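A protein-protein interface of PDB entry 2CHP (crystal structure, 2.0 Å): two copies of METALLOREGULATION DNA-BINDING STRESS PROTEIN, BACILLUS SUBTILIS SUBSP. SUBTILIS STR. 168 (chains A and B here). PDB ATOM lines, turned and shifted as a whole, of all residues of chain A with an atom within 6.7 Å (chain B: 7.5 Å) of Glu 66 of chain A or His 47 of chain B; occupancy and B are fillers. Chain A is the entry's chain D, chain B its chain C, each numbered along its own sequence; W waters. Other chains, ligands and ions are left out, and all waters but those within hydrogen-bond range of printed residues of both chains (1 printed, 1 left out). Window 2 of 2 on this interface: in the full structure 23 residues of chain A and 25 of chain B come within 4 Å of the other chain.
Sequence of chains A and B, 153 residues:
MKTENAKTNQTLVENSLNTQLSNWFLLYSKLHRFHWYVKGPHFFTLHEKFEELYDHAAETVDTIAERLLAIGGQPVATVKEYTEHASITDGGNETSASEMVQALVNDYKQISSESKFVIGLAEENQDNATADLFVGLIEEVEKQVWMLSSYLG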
ATOM      1  N   THR A  60      38.386  18.927   7.188  1.00  0.00           N
ATOM      2  CA  THR A  60      38.160  19.510   8.509  1.00  0.00           C
ATOM      3  C   THR A  60      36.851  20.281   8.559  1.00  0.00           C
ATOM      4  O   THR A  60      36.086  20.155   9.530  1.00  0.00           O
ATOM      5  CB  THR A  60      39.377  20.390   8.923  1.00  0.00           C
ATOM      6  OG1 THR A  60      40.586  19.642   8.801  1.00  0.00           O
ATOM      7  CG2 THR A  60      39.290  20.926  10.373  1.00  0.00           C
ATOM      8  N   VAL A  61      36.583  21.104   7.557  1.00  0.00           N
ATOM      9  CA  VAL A  61      35.301  21.814   7.459  1.00  0.00           C
ATOM     10  C   VAL A  61      34.122  20.816   7.610  1.00  0.00           C
ATOM     11  O   VAL A  61      33.201  21.011   8.413  1.00  0.00           O
ATOM     12  CB  VAL A  61      35.206  22.543   6.076  1.00  0.00           C
ATOM     13  CG1 VAL A  61      33.758  22.926   5.677  1.00  0.00           C
ATOM     14  CG2 VAL A  61      36.077  23.758   6.027  1.00  0.00           C
ATOM     15  N   ASP A  62      34.154  19.750   6.835  1.00  0.00           N
ATOM     16  CA  ASP A  62      33.044  18.803   6.848  1.00  0.00           C
ATOM     17  C   ASP A  62      32.955  18.085   8.199  1.00  0.00           C
ATOM     18  O   ASP A  62      31.847  17.958   8.735  1.00  0.00           O
ATOM     19  CB  ASP A  62      33.157  17.805   5.714  1.00  0.00           C
ATOM     20  CG  ASP A  62      31.846  16.940   5.541  1.00  0.00           C
ATOM     21  OD1 ASP A  62      30.699  17.470   5.720  1.00  0.00           O
ATOM     22  OD2 ASP A  62      31.996  15.717   5.247  1.00  0.00           O
ATOM     23  N   THR A  63      34.074  17.719   8.811  1.00  0.00           N
ATOM     24  CA  THR A  63      34.069  17.023  10.119  1.00  0.00           C
ATOM     25  C   THR A  63      33.543  17.898  11.305  1.00  0.00           C
ATOM     26  O   THR A  63      32.744  17.439  12.121  1.00  0.00           O
ATOM     27  CB  THR A  63      35.474  16.538  10.411  1.00  0.00           C
ATOM     28  OG1 THR A  63      35.833  15.538   9.413  1.00  0.00           O
ATOM     29  CG2 THR A  63      35.590  15.965  11.763  1.00  0.00           C
ATOM     30  N   ILE A  64      33.965  19.167  11.369  1.00  0.00           N
ATOM     31  CA  ILE A  64      33.398  20.118  12.330  1.00  0.00           C
ATOM     32  C   ILE A  64      31.904  20.328  12.167  1.00  0.00           C
ATOM     33  O   ILE A  64      31.137  20.244  13.158  1.00  0.00           O
ATOM     34  CB  ILE A  64      34.144  21.475  12.323  1.00  0.00           C
ATOM     35  CG1 ILE A  64      35.607  21.263  12.711  1.00  0.00           C
ATOM     36  CG2 ILE A  64      33.452  22.511  13.254  1.00  0.00           C
ATOM     37  CD1 ILE A  64      36.596  22.498  12.591  1.00  0.00           C
ATOM     38  N   ALA A  65      31.456  20.659  10.944  1.00  0.00           N
ATOM     39  CA  ALA A  65      30.072  20.878  10.685  1.00  0.00           C
ATOM     40  C   ALA A  65      29.285  19.641  11.102  1.00  0.00           C
ATOM     41  O   ALA A  65      28.193  19.771  11.669  1.00  0.00           O
ATOM     42  CB  ALA A  65      29.804  21.216   9.186  1.00  0.00           C
ATOM     43  N   GLU A  66      29.743  18.463  10.745  1.00  0.00           N
ATOM     44  CA  GLU A  66      28.947  17.290  11.045  1.00  0.00           C
ATOM     45  C   GLU A  66      28.962  16.956  12.513  1.00  0.00           C
ATOM     46  O   GLU A  66      27.991  16.439  12.997  1.00  0.00           O
ATOM     47  CB  GLU A  66      29.327  16.082  10.143  1.00  0.00           C
ATOM     48  CG  GLU A  66      28.954  16.476   8.661  1.00  0.00           C
ATOM     49  CD  GLU A  66      28.662  15.335   7.678  1.00  0.00           C
ATOM     50  OE1 GLU A  66      27.953  15.721   6.676  1.00  0.00           O
ATOM     51  OE2 GLU A  66      29.118  14.144   7.928  1.00  0.00           O
ATOM     52  N   ARG A  67      30.028  17.274  13.247  1.00  0.00           N
ATOM     53  CA  ARG A  67      29.964  17.127  14.716  1.00  0.00           C
ATOM     54  C   ARG A  67      28.953  18.151  15.316  1.00  0.00           C
ATOM     55  O   ARG A  67      28.144  17.763  16.177  1.00  0.00           O
ATOM     56  CB  ARG A  67      31.320  17.251  15.379  1.00  0.00           C
ATOM     57  CG  ARG A  67      31.325  17.087  16.921  1.00  0.00           C
ATOM     58  CD  ARG A  67      30.986  15.710  17.334  1.00  0.00           C
ATOM     59  NE  ARG A  67      30.772  15.600  18.756  1.00  0.00           N
ATOM     60  CZ  ARG A  67      29.945  14.721  19.357  1.00  0.00           C
ATOM     61  NH1 ARG A  67      29.284  13.777  18.653  1.00  0.00           N
ATOM     62  NH2 ARG A  67      29.768  14.780  20.688  1.00  0.00           N
ATOM     63  N   LEU A  68      29.003  19.409  14.865  1.00  0.00           N
ATOM     64  CA  LEU A  68      28.011  20.430  15.316  1.00  0.00           C
ATOM     65  C   LEU A  68      26.566  19.926  15.117  1.00  0.00           C
ATOM     66  O   LEU A  68      25.692  20.082  15.994  1.00  0.00           O
ATOM     67  CB  LEU A  68      28.148  21.751  14.548  1.00  0.00           C
ATOM     68  CG  LEU A  68      27.954  23.093  15.294  1.00  0.00           C
ATOM     69  CD1 LEU A  68      27.657  24.303  14.389  1.00  0.00           C
ATOM     70  CD2 LEU A  68      27.153  23.007  16.611  1.00  0.00           C
ATOM     71  N   LEU A  69      26.288  19.386  13.946  1.00  0.00           N
ATOM     72  CA  LEU A  69      24.974  18.781  13.662  1.00  0.00           C
ATOM     73  C   LEU A  69      24.642  17.644  14.662  1.00  0.00           C
ATOM     74  O   LEU A  69      23.538  17.539  15.245  1.00  0.00           O
ATOM     75  CB  LEU A  69      24.980  18.290  12.239  1.00  0.00           C
ATOM     76  CG  LEU A  69      24.517  19.052  10.981  1.00  0.00           C
ATOM     77  CD1 LEU A  69      23.660  20.273  11.134  1.00  0.00           C
ATOM     78  CD2 LEU A  69      25.585  19.063   9.891  1.00  0.00           C
ATOM     79  N   ALA A  70      25.614  16.776  14.858  1.00  0.00           N
ATOM     80  CA  ALA A  70      25.426  15.643  15.724  1.00  0.00           C
ATOM     81  C   ALA A  70      25.103  16.026  17.224  1.00  0.00           C
ATOM     82  O   ALA A  70      24.417  15.259  17.970  1.00  0.00           O
ATOM     83  CB  ALA A  70      26.637  14.751  15.629  1.00  0.00           C
ATOM     84  N   ILE A  71      25.569  17.190  17.664  1.00  0.00           N
ATOM     85  CA  ILE A  71      25.254  17.654  19.023  1.00  0.00           C
ATOM     86  C   ILE A  71      24.011  18.495  19.108  1.00  0.00           C
ATOM     87  O   ILE A  71      23.645  18.891  20.210  1.00  0.00           O
ATOM     88  CB  ILE A  71      26.439  18.315  19.737  1.00  0.00           C
ATOM     89  CG1 ILE A  71      26.818  19.664  19.103  1.00  0.00           C
ATOM     90  CG2 ILE A  71      27.634  17.282  19.832  1.00  0.00           C
ATOM     91  CD1 ILE A  71      28.071  20.354  19.864  1.00  0.00           C
ATOM     92  N   PRO A  75      25.280  24.618  11.957  1.00  0.00           N
ATOM     93  CA  PRO A  75      26.454  25.177  11.350  1.00  0.00           C
ATOM     94  C   PRO A  75      26.131  26.321  10.381  1.00  0.00           C
ATOM     95  O   PRO A  75      25.203  26.282   9.565  1.00  0.00           O
ATOM     96  CB  PRO A  75      27.067  23.976  10.531  1.00  0.00           C
ATOM     97  CG  PRO A  75      25.970  22.965  10.392  1.00  0.00           C
ATOM     98  CD  PRO A  75      25.020  23.208  11.547  1.00  0.00           C
ATOM     99  N   LEU A 133      37.940  15.445  18.758  1.00  0.00           N
ATOM    100  CA  LEU A 133      38.001  16.030  17.421  1.00  0.00           C
ATOM    101  C   LEU A 133      39.043  17.132  17.294  1.00  0.00           C
ATOM    102  O   LEU A 133      39.943  17.132  16.407  1.00  0.00           O
ATOM    103  CB  LEU A 133      36.620  16.576  17.022  1.00  0.00           C
ATOM    104  CG  LEU A 133      36.485  17.363  15.693  1.00  0.00           C
ATOM    105  CD1 LEU A 133      37.337  16.726  14.724  1.00  0.00           C
ATOM    106  CD2 LEU A 133      34.985  17.426  15.223  1.00  0.00           C
ATOM    107  N   LEU B  31      26.404  24.179  -2.015  1.00  0.00           N
ATOM    108  CA  LEU B  31      26.333  22.732  -1.943  1.00  0.00           C
ATOM    109  C   LEU B  31      26.675  22.147  -0.561  1.00  0.00           C
ATOM    110  O   LEU B  31      26.101  21.142  -0.189  1.00  0.00           O
ATOM    111  CB  LEU B  31      27.236  22.115  -3.027  1.00  0.00           C
ATOM    112  CG  LEU B  31      26.680  22.238  -4.444  1.00  0.00           C
ATOM    113  CD1 LEU B  31      27.849  22.091  -5.561  1.00  0.00           C
ATOM    114  CD2 LEU B  31      25.566  21.137  -4.613  1.00  0.00           C
ATOM    115  N   HIS B  32      27.602  22.765   0.187  1.00  0.00           N
ATOM    116  CA  HIS B  32      27.844  22.412   1.611  1.00  0.00           C
ATOM    117  C   HIS B  32      26.626  22.721   2.494  1.00  0.00           C
ATOM    118  O   HIS B  32      26.207  21.835   3.260  1.00  0.00           O
ATOM    119  CB  HIS B  32      29.091  23.158   2.178  1.00  0.00           C
ATOM    120  CG  HIS B  32      30.369  22.553   1.740  1.00  0.00           C
ATOM    121  ND1 HIS B  32      30.824  22.639   0.424  1.00  0.00           N
ATOM    122  CD2 HIS B  32      31.209  21.701   2.381  1.00  0.00           C
ATOM    123  CE1 HIS B  32      31.967  21.968   0.331  1.00  0.00           C
ATOM    124  NE2 HIS B  32      32.229  21.399   1.512  1.00  0.00           N
ATOM    125  N   PHE B  34      23.452  22.698   1.585  1.00  0.00           N
ATOM    126  CA  PHE B  34      22.443  21.686   1.266  1.00  0.00           C
ATOM    127  C   PHE B  34      22.843  20.279   1.749  1.00  0.00           C
ATOM    128  O   PHE B  34      21.984  19.523   2.218  1.00  0.00           O
ATOM    129  CB  PHE B  34      22.194  21.631  -0.256  1.00  0.00           C
ATOM    130  CG  PHE B  34      21.611  22.924  -0.858  1.00  0.00           C
ATOM    131  CD1 PHE B  34      21.477  23.054  -2.220  1.00  0.00           C
ATOM    132  CD2 PHE B  34      21.110  23.967  -0.029  1.00  0.00           C
ATOM    133  CE1 PHE B  34      20.927  24.244  -2.764  1.00  0.00           C
ATOM    134  CE2 PHE B  34      20.520  25.127  -0.563  1.00  0.00           C
ATOM    135  CZ  PHE B  34      20.452  25.274  -1.930  1.00  0.00           C
ATOM    136  N   HIS B  35      24.133  19.937   1.631  1.00  0.00           N
ATOM    137  CA  HIS B  35      24.716  18.681   2.149  1.00  0.00           C
ATOM    138  C   HIS B  35      24.452  18.561   3.647  1.00  0.00           C
ATOM    139  O   HIS B  35      24.207  17.445   4.156  1.00  0.00           O
ATOM    140  CB  HIS B  35      26.217  18.726   1.879  1.00  0.00           C
ATOM    141  CG  HIS B  35      27.028  17.585   2.416  1.00  0.00           C
ATOM    142  ND1 HIS B  35      26.950  16.295   1.918  1.00  0.00           N
ATOM    143  CD2 HIS B  35      27.994  17.560   3.359  1.00  0.00           C
ATOM    144  CE1 HIS B  35      27.850  15.530   2.521  1.00  0.00           C
ATOM    145  NE2 HIS B  35      28.511  16.287   3.383  1.00  0.00           N
ATOM    146  N   TRP B  36      24.540  19.684   4.372  1.00  0.00           N
ATOM    147  CA  TRP B  36      24.425  19.686   5.847  1.00  0.00           C
ATOM    148  C   TRP B  36      22.994  19.770   6.331  1.00  0.00           C
ATOM    149  O   TRP B  36      22.691  19.244   7.432  1.00  0.00           O
ATOM    150  CB  TRP B  36      25.204  20.864   6.449  1.00  0.00           C
ATOM    151  CG  TRP B  36      26.691  20.743   6.290  1.00  0.00           C
ATOM    152  CD1 TRP B  36      27.427  19.599   6.280  1.00  0.00           C
ATOM    153  CD2 TRP B  36      27.614  21.808   6.208  1.00  0.00           C
ATOM    154  NE1 TRP B  36      28.720  19.884   6.065  1.00  0.00           N
ATOM    155  CE2 TRP B  36      28.885  21.237   6.059  1.00  0.00           C
ATOM    156  CE3 TRP B  36      27.487  23.203   6.150  1.00  0.00           C
ATOM    157  CZ2 TRP B  36      30.028  22.002   5.915  1.00  0.00           C
ATOM    158  CZ3 TRP B  36      28.637  23.970   6.059  1.00  0.00           C
ATOM    159  CH2 TRP B  36      29.879  23.369   5.932  1.00  0.00           C
ATOM    160  N   TYR B  37      22.131  20.452   5.571  1.00  0.00           N
ATOM    161  CA  TYR B  37      20.781  20.723   6.059  1.00  0.00           C
ATOM    162  C   TYR B  37      19.680  19.880   5.412  1.00  0.00           C
ATOM    163  O   TYR B  37      18.542  19.919   5.860  1.00  0.00           O
ATOM    164  CB  TYR B  37      20.476  22.199   5.965  1.00  0.00           C
ATOM    165  CG  TYR B  37      21.135  23.029   7.042  1.00  0.00           C
ATOM    166  CD1 TYR B  37      20.488  23.204   8.300  1.00  0.00           C
ATOM    167  CD2 TYR B  37      22.377  23.640   6.847  1.00  0.00           C
ATOM    168  CE1 TYR B  37      21.081  23.960   9.335  1.00  0.00           C
ATOM    169  CE2 TYR B  37      22.959  24.430   7.868  1.00  0.00           C
ATOM    170  CZ  TYR B  37      22.312  24.575   9.098  1.00  0.00           C
ATOM    171  OH  TYR B  37      22.889  25.305  10.105  1.00  0.00           O
ATOM    172  N   VAL B  38      19.987  19.092   4.395  1.00  0.00           N
ATOM    173  CA  VAL B  38      18.929  18.296   3.742  1.00  0.00           C
ATOM    174  C   VAL B  38      18.290  17.361   4.740  1.00  0.00           C
ATOM    175  O   VAL B  38      18.957  16.883   5.610  1.00  0.00           O
ATOM    176  CB  VAL B  38      19.473  17.522   2.447  1.00  0.00           C
ATOM    177  CG1 VAL B  38      20.667  16.532   2.843  1.00  0.00           C
ATOM    178  CG2 VAL B  38      18.260  16.920   1.604  1.00  0.00           C
ATOM    179  N   HIS B  42      14.660  11.231   1.554  1.00  0.00           N
ATOM    180  CA  HIS B  42      15.726  11.214   0.528  1.00  0.00           C
ATOM    181  C   HIS B  42      17.060  11.746   1.054  1.00  0.00           C
ATOM    182  O   HIS B  42      17.990  11.970   0.242  1.00  0.00           O
ATOM    183  CB  HIS B  42      15.277  11.992  -0.667  1.00  0.00           C
ATOM    184  CG  HIS B  42      13.904  11.588  -1.137  1.00  0.00           C
ATOM    185  ND1 HIS B  42      13.646  10.352  -1.715  1.00  0.00           N
ATOM    186  CD2 HIS B  42      12.720  12.227  -1.065  1.00  0.00           C
ATOM    187  CE1 HIS B  42      12.351  10.263  -1.985  1.00  0.00           C
ATOM    188  NE2 HIS B  42      11.768  11.374  -1.585  1.00  0.00           N
ATOM    189  N   PHE B  43      17.184  11.888   2.389  1.00  0.00           N
ATOM    190  CA  PHE B  43      18.440  12.263   3.018  1.00  0.00           C
ATOM    191  C   PHE B  43      19.704  11.575   2.495  1.00  0.00           C
ATOM    192  O   PHE B  43      20.692  12.260   2.190  1.00  0.00           O
ATOM    193  CB  PHE B  43      18.413  12.070   4.558  1.00  0.00           C
ATOM    194  CG  PHE B  43      19.728  12.409   5.209  1.00  0.00           C
ATOM    195  CD1 PHE B  43      20.085  13.722   5.428  1.00  0.00           C
ATOM    196  CD2 PHE B  43      20.677  11.421   5.457  1.00  0.00           C
ATOM    197  CE1 PHE B  43      21.358  14.027   5.981  1.00  0.00           C
ATOM    198  CE2 PHE B  43      21.925  11.710   5.982  1.00  0.00           C
ATOM    199  CZ  PHE B  43      22.279  13.028   6.240  1.00  0.00           C
ATOM    200  N   PHE B  44      19.755  10.244   2.473  1.00  0.00           N
ATOM    201  CA  PHE B  44      21.008   9.560   2.184  1.00  0.00           C
ATOM    202  C   PHE B  44      21.453   9.874   0.734  1.00  0.00           C
ATOM    203  O   PHE B  44      22.589  10.301   0.505  1.00  0.00           O
ATOM    204  CB  PHE B  44      20.925   8.058   2.494  1.00  0.00           C
ATOM    205  CG  PHE B  44      20.844   7.755   3.966  1.00  0.00           C
ATOM    206  CD1 PHE B  44      21.951   7.964   4.808  1.00  0.00           C
ATOM    207  CD2 PHE B  44      19.618   7.428   4.532  1.00  0.00           C
ATOM    208  CE1 PHE B  44      21.898   7.666   6.151  1.00  0.00           C
ATOM    209  CE2 PHE B  44      19.514   7.189   5.896  1.00  0.00           C
ATOM    210  CZ  PHE B  44      20.671   7.323   6.701  1.00  0.00           C
ATOM    211  N   THR B  45      20.519   9.758  -0.195  1.00  0.00           N
ATOM    212  CA  THR B  45      20.778   9.997  -1.606  1.00  0.00           C
ATOM    213  C   THR B  45      21.307  11.395  -1.854  1.00  0.00           C
ATOM    214  O   THR B  45      22.361  11.584  -2.450  1.00  0.00           O
ATOM    215  CB  THR B  45      19.513   9.705  -2.400  1.00  0.00           C
ATOM    216  OG1 THR B  45      19.318   8.283  -2.346  1.00  0.00           O
ATOM    217  CG2 THR B  45      19.692  10.062  -3.888  1.00  0.00           C
ATOM    218  N   LEU B  46      20.581  12.390  -1.333  1.00  0.00           N
ATOM    219  CA  LEU B  46      20.914  13.779  -1.584  1.00  0.00           C
ATOM    220  C   LEU B  46      22.101  14.257  -0.791  1.00  0.00           C
ATOM    221  O   LEU B  46      22.870  15.084  -1.279  1.00  0.00           O
ATOM    222  CB  LEU B  46      19.685  14.648  -1.393  1.00  0.00           C
ATOM    223  CG  LEU B  46      18.466  14.481  -2.301  1.00  0.00           C
ATOM    224  CD1 LEU B  46      17.326  15.393  -1.827  1.00  0.00           C
ATOM    225  CD2 LEU B  46      18.811  14.741  -3.796  1.00  0.00           C
ATOM    226  N   HIS B  47      22.280  13.799   0.446  1.00  0.00           N
ATOM    227  CA  HIS B  47      23.508  14.155   1.213  1.00  0.00           C
ATOM    228  C   HIS B  47      24.773  13.710   0.429  1.00  0.00           C
ATOM    229  O   HIS B  47      25.774  14.448   0.287  1.00  0.00           O
ATOM    230  CB  HIS B  47      23.402  13.479   2.599  1.00  0.00           C
ATOM    231  CG  HIS B  47      24.640  13.576   3.454  1.00  0.00           C
ATOM    232  ND1 HIS B  47      24.950  14.705   4.176  1.00  0.00           N
ATOM    233  CD2 HIS B  47      25.574  12.655   3.781  1.00  0.00           C
ATOM    234  CE1 HIS B  47      26.047  14.488   4.882  1.00  0.00           C
ATOM    235  NE2 HIS B  47      26.471  13.266   4.628  1.00  0.00           N
ATOM    236  N   GLU B  48      24.711  12.532  -0.158  1.00  0.00           N
ATOM    237  CA  GLU B  48      25.830  12.016  -0.985  1.00  0.00           C
ATOM    238  C   GLU B  48      25.930  12.734  -2.325  1.00  0.00           C
ATOM    239  O   GLU B  48      27.004  13.101  -2.727  1.00  0.00           O
ATOM    240  CB  GLU B  48      25.701  10.504  -1.211  1.00  0.00           C
ATOM    241  CG  GLU B  48      25.837   9.724   0.074  1.00  0.00           C
ATOM    242  CD  GLU B  48      25.155   8.306   0.073  1.00  0.00           C
ATOM    243  OE1 GLU B  48      24.879   7.771  -1.045  1.00  0.00           O
ATOM    244  OE2 GLU B  48      24.924   7.752   1.209  1.00  0.00           O
ATOM    245  N   LYS B  49      24.820  12.960  -3.005  1.00  0.00           N
ATOM    246  CA  LYS B  49      24.858  13.655  -4.318  1.00  0.00           C
ATOM    247  C   LYS B  49      25.423  15.065  -4.207  1.00  0.00           C
ATOM    248  O   LYS B  49      26.228  15.475  -4.984  1.00  0.00           O
ATOM    249  CB  LYS B  49      23.471  13.715  -4.938  1.00  0.00           C
ATOM    250  CG  LYS B  49      23.351  14.379  -6.295  1.00  0.00           C
ATOM    251  CD  LYS B  49      24.155  13.643  -7.383  1.00  0.00           C
ATOM    252  CE  LYS B  49      24.047  14.380  -8.730  1.00  0.00           C
ATOM    253  NZ  LYS B  49      24.820  13.735  -9.895  1.00  0.00           N
ATOM    254  N   PHE B  50      24.993  15.806  -3.198  1.00  0.00           N
ATOM    255  CA  PHE B  50      25.560  17.133  -2.948  1.00  0.00           C
ATOM    256  C   PHE B  50      27.050  17.146  -2.684  1.00  0.00           C
ATOM    257  O   PHE B  50      27.721  18.069  -3.154  1.00  0.00           O
ATOM    258  CB  PHE B  50      24.792  17.857  -1.817  1.00  0.00           C
ATOM    259  CG  PHE B  50      23.330  18.052  -2.096  1.00  0.00           C
ATOM    260  CD1 PHE B  50      22.419  18.154  -1.035  1.00  0.00           C
ATOM    261  CD2 PHE B  50      22.837  18.161  -3.385  1.00  0.00           C
ATOM    262  CE1 PHE B  50      21.073  18.318  -1.224  1.00  0.00           C
ATOM    263  CE2 PHE B  50      21.422  18.345  -3.581  1.00  0.00           C
ATOM    264  CZ  PHE B  50      20.577  18.441  -2.472  1.00  0.00           C
ATOM    265  N   GLU B  51      27.586  16.159  -1.967  1.00  0.00           N
ATOM    266  CA  GLU B  51      29.038  16.037  -1.830  1.00  0.00           C
ATOM    267  C   GLU B  51      29.736  15.760  -3.155  1.00  0.00           C
ATOM    268  O   GLU B  51      30.758  16.369  -3.470  1.00  0.00           O
ATOM    269  CB  GLU B  51      29.438  14.937  -0.829  1.00  0.00           C
ATOM    270  CG  GLU B  51      30.969  14.816  -0.700  1.00  0.00           C
ATOM    271  CD  GLU B  51      31.423  13.904   0.479  1.00  0.00           C
ATOM    272  OE1 GLU B  51      30.575  13.509   1.284  1.00  0.00           O
ATOM    273  OE2 GLU B  51      32.631  13.635   0.602  1.00  0.00           O
ATOM    274  N   GLU B  52      29.206  14.830  -3.949  1.00  0.00           N
ATOM    275  CA  GLU B  52      29.800  14.590  -5.305  1.00  0.00           C
ATOM    276  C   GLU B  52      29.881  15.915  -6.103  1.00  0.00           C
ATOM    277  O   GLU B  52      30.864  16.174  -6.811  1.00  0.00           O
ATOM    278  CB  GLU B  52      28.998  13.528  -6.106  1.00  0.00           C
ATOM    279  CG  GLU B  52      29.188  12.150  -5.502  1.00  0.00           C
ATOM    280  CD  GLU B  52      28.220  11.072  -6.064  1.00  0.00           C
ATOM    281  OE1 GLU B  52      27.420  11.326  -7.026  1.00  0.00           O
ATOM    282  OE2 GLU B  52      28.281   9.930  -5.507  1.00  0.00           O
ATOM    283  N   LEU B  53      28.806  16.685  -6.046  1.00  0.00           N
ATOM    284  CA  LEU B  53      28.700  17.947  -6.843  1.00  0.00           C
ATOM    285  C   LEU B  53      29.688  19.013  -6.346  1.00  0.00           C
ATOM    286  O   LEU B  53      30.253  19.754  -7.127  1.00  0.00           O
ATOM    287  CB  LEU B  53      27.236  18.455  -6.821  1.00  0.00           C
ATOM    288  CG  LEU B  53      26.202  17.607  -7.614  1.00  0.00           C
ATOM    289  CD1 LEU B  53      24.744  18.187  -7.442  1.00  0.00           C
ATOM    290  CD2 LEU B  53      26.555  17.489  -9.103  1.00  0.00           C
ATOM    291  N   TYR B  54      29.935  19.049  -5.022  1.00  0.00           N
ATOM    292  CA  TYR B  54      30.871  20.039  -4.544  1.00  0.00           C
ATOM    293  C   TYR B  54      32.290  19.657  -4.804  1.00  0.00           C
ATOM    294  O   TYR B  54      33.106  20.516  -5.032  1.00  0.00           O
ATOM    295  CB  TYR B  54      30.571  20.530  -3.118  1.00  0.00           C
ATOM    296  CG  TYR B  54      30.758  19.631  -1.910  1.00  0.00           C
ATOM    297  CD1 TYR B  54      31.954  19.042  -1.604  1.00  0.00           C
ATOM    298  CD2 TYR B  54      29.763  19.586  -0.943  1.00  0.00           C
ATOM    299  CE1 TYR B  54      32.120  18.268  -0.415  1.00  0.00           C
ATOM    300  CE2 TYR B  54      29.911  18.875   0.199  1.00  0.00           C
ATOM    301  CZ  TYR B  54      31.101  18.230   0.486  1.00  0.00           C
ATOM    302  OH  TYR B  54      31.223  17.512   1.671  1.00  0.00           O
HETATM  303  O   HOH W   1      28.887  12.440   5.973  1.00  0.00           O
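Trp 36 of chain B touches Val 61 of chain A.
OH of Tyr 54 of chain B touches CG of Asp 62 of chain A, 3.96 Å away.
CB of Ala 65 of chain A touches CE2 of Trp 36 of chain B, at 3.3 Å.
Trp 36 of chain B touches Glu 66 of chain A.
Glu 66 of chain A touches His 47 of chain B (OE1 to CE1, 2.9 Å).
Trp 36 of chain B touches Leu 69 of chain A.
Of chain A, only Glu 66 (2.9 Å) comes within 4 Å of His 47 of chain B.
Printed residues of chain B within 4 Å of Asp 62 of chain A: His 35, Trp 36 and Tyr 54.
Of the printed residues of chain A, Tyr 37 of chain B touches Pro 75 (2.6 Å).
Of the printed residues of chain B, Leu 69 of chain A touches Trp 36 (3.8 Å).
Val 38 of chain B touches none of the printed residues of chain A.
The nearest printed residue of chain B that does not touch Pro 75 of chain A is Trp 36 of chain B (4.5 Å).
Hydrophobic or aromatic side chains of chain B that line the printed part of chain A: His 35, Trp 36, Tyr 37, His 47 and Tyr 54.
Of the 14 printed residues of chain A, 6 touch a printed residue of chain B.
Among the printed residues, 10 pairs touch across the chains.
No position is printed for both chains.
A ring nitrogen (ND1) of His 35 of chain B is in hydrogen-bond range of the backbone carbonyl oxygen (O) of His 47 of chain B (2.7 Å).
OH of Tyr 54 of chain B is in hydrogen-bond range of NE2 of His 35 of chain B (3.4 Å).
Water W1 bridges the side-chain carboxylate (OE2) of Glu 66 of chain A (2.6 Å) and a ring nitrogen (NE2) of His 47 of chain B (2.9 Å).
The side-chain carboxylate of Asp 62 of chain A sits at hydrogen-bond distance from a ring nitrogen (NE2) of His 35 of chain B (3.4 Å).
NE2 of His 35 of chain B is in hydrogen-bond range of OE1 of Glu 66 of chain A (3.4 Å).
The backbone carbonyl oxygen (O) of Pro 75 of chain A is in hydrogen-bond range of the side-chain hydroxyl (OH) of Tyr 37 of chain B (2.6 Å).
The indole nitrogen of Trp 36 of chain B sits at hydrogen-bond distance from the side-chain carboxylate of Asp 62 of chain A (3.1 Å).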
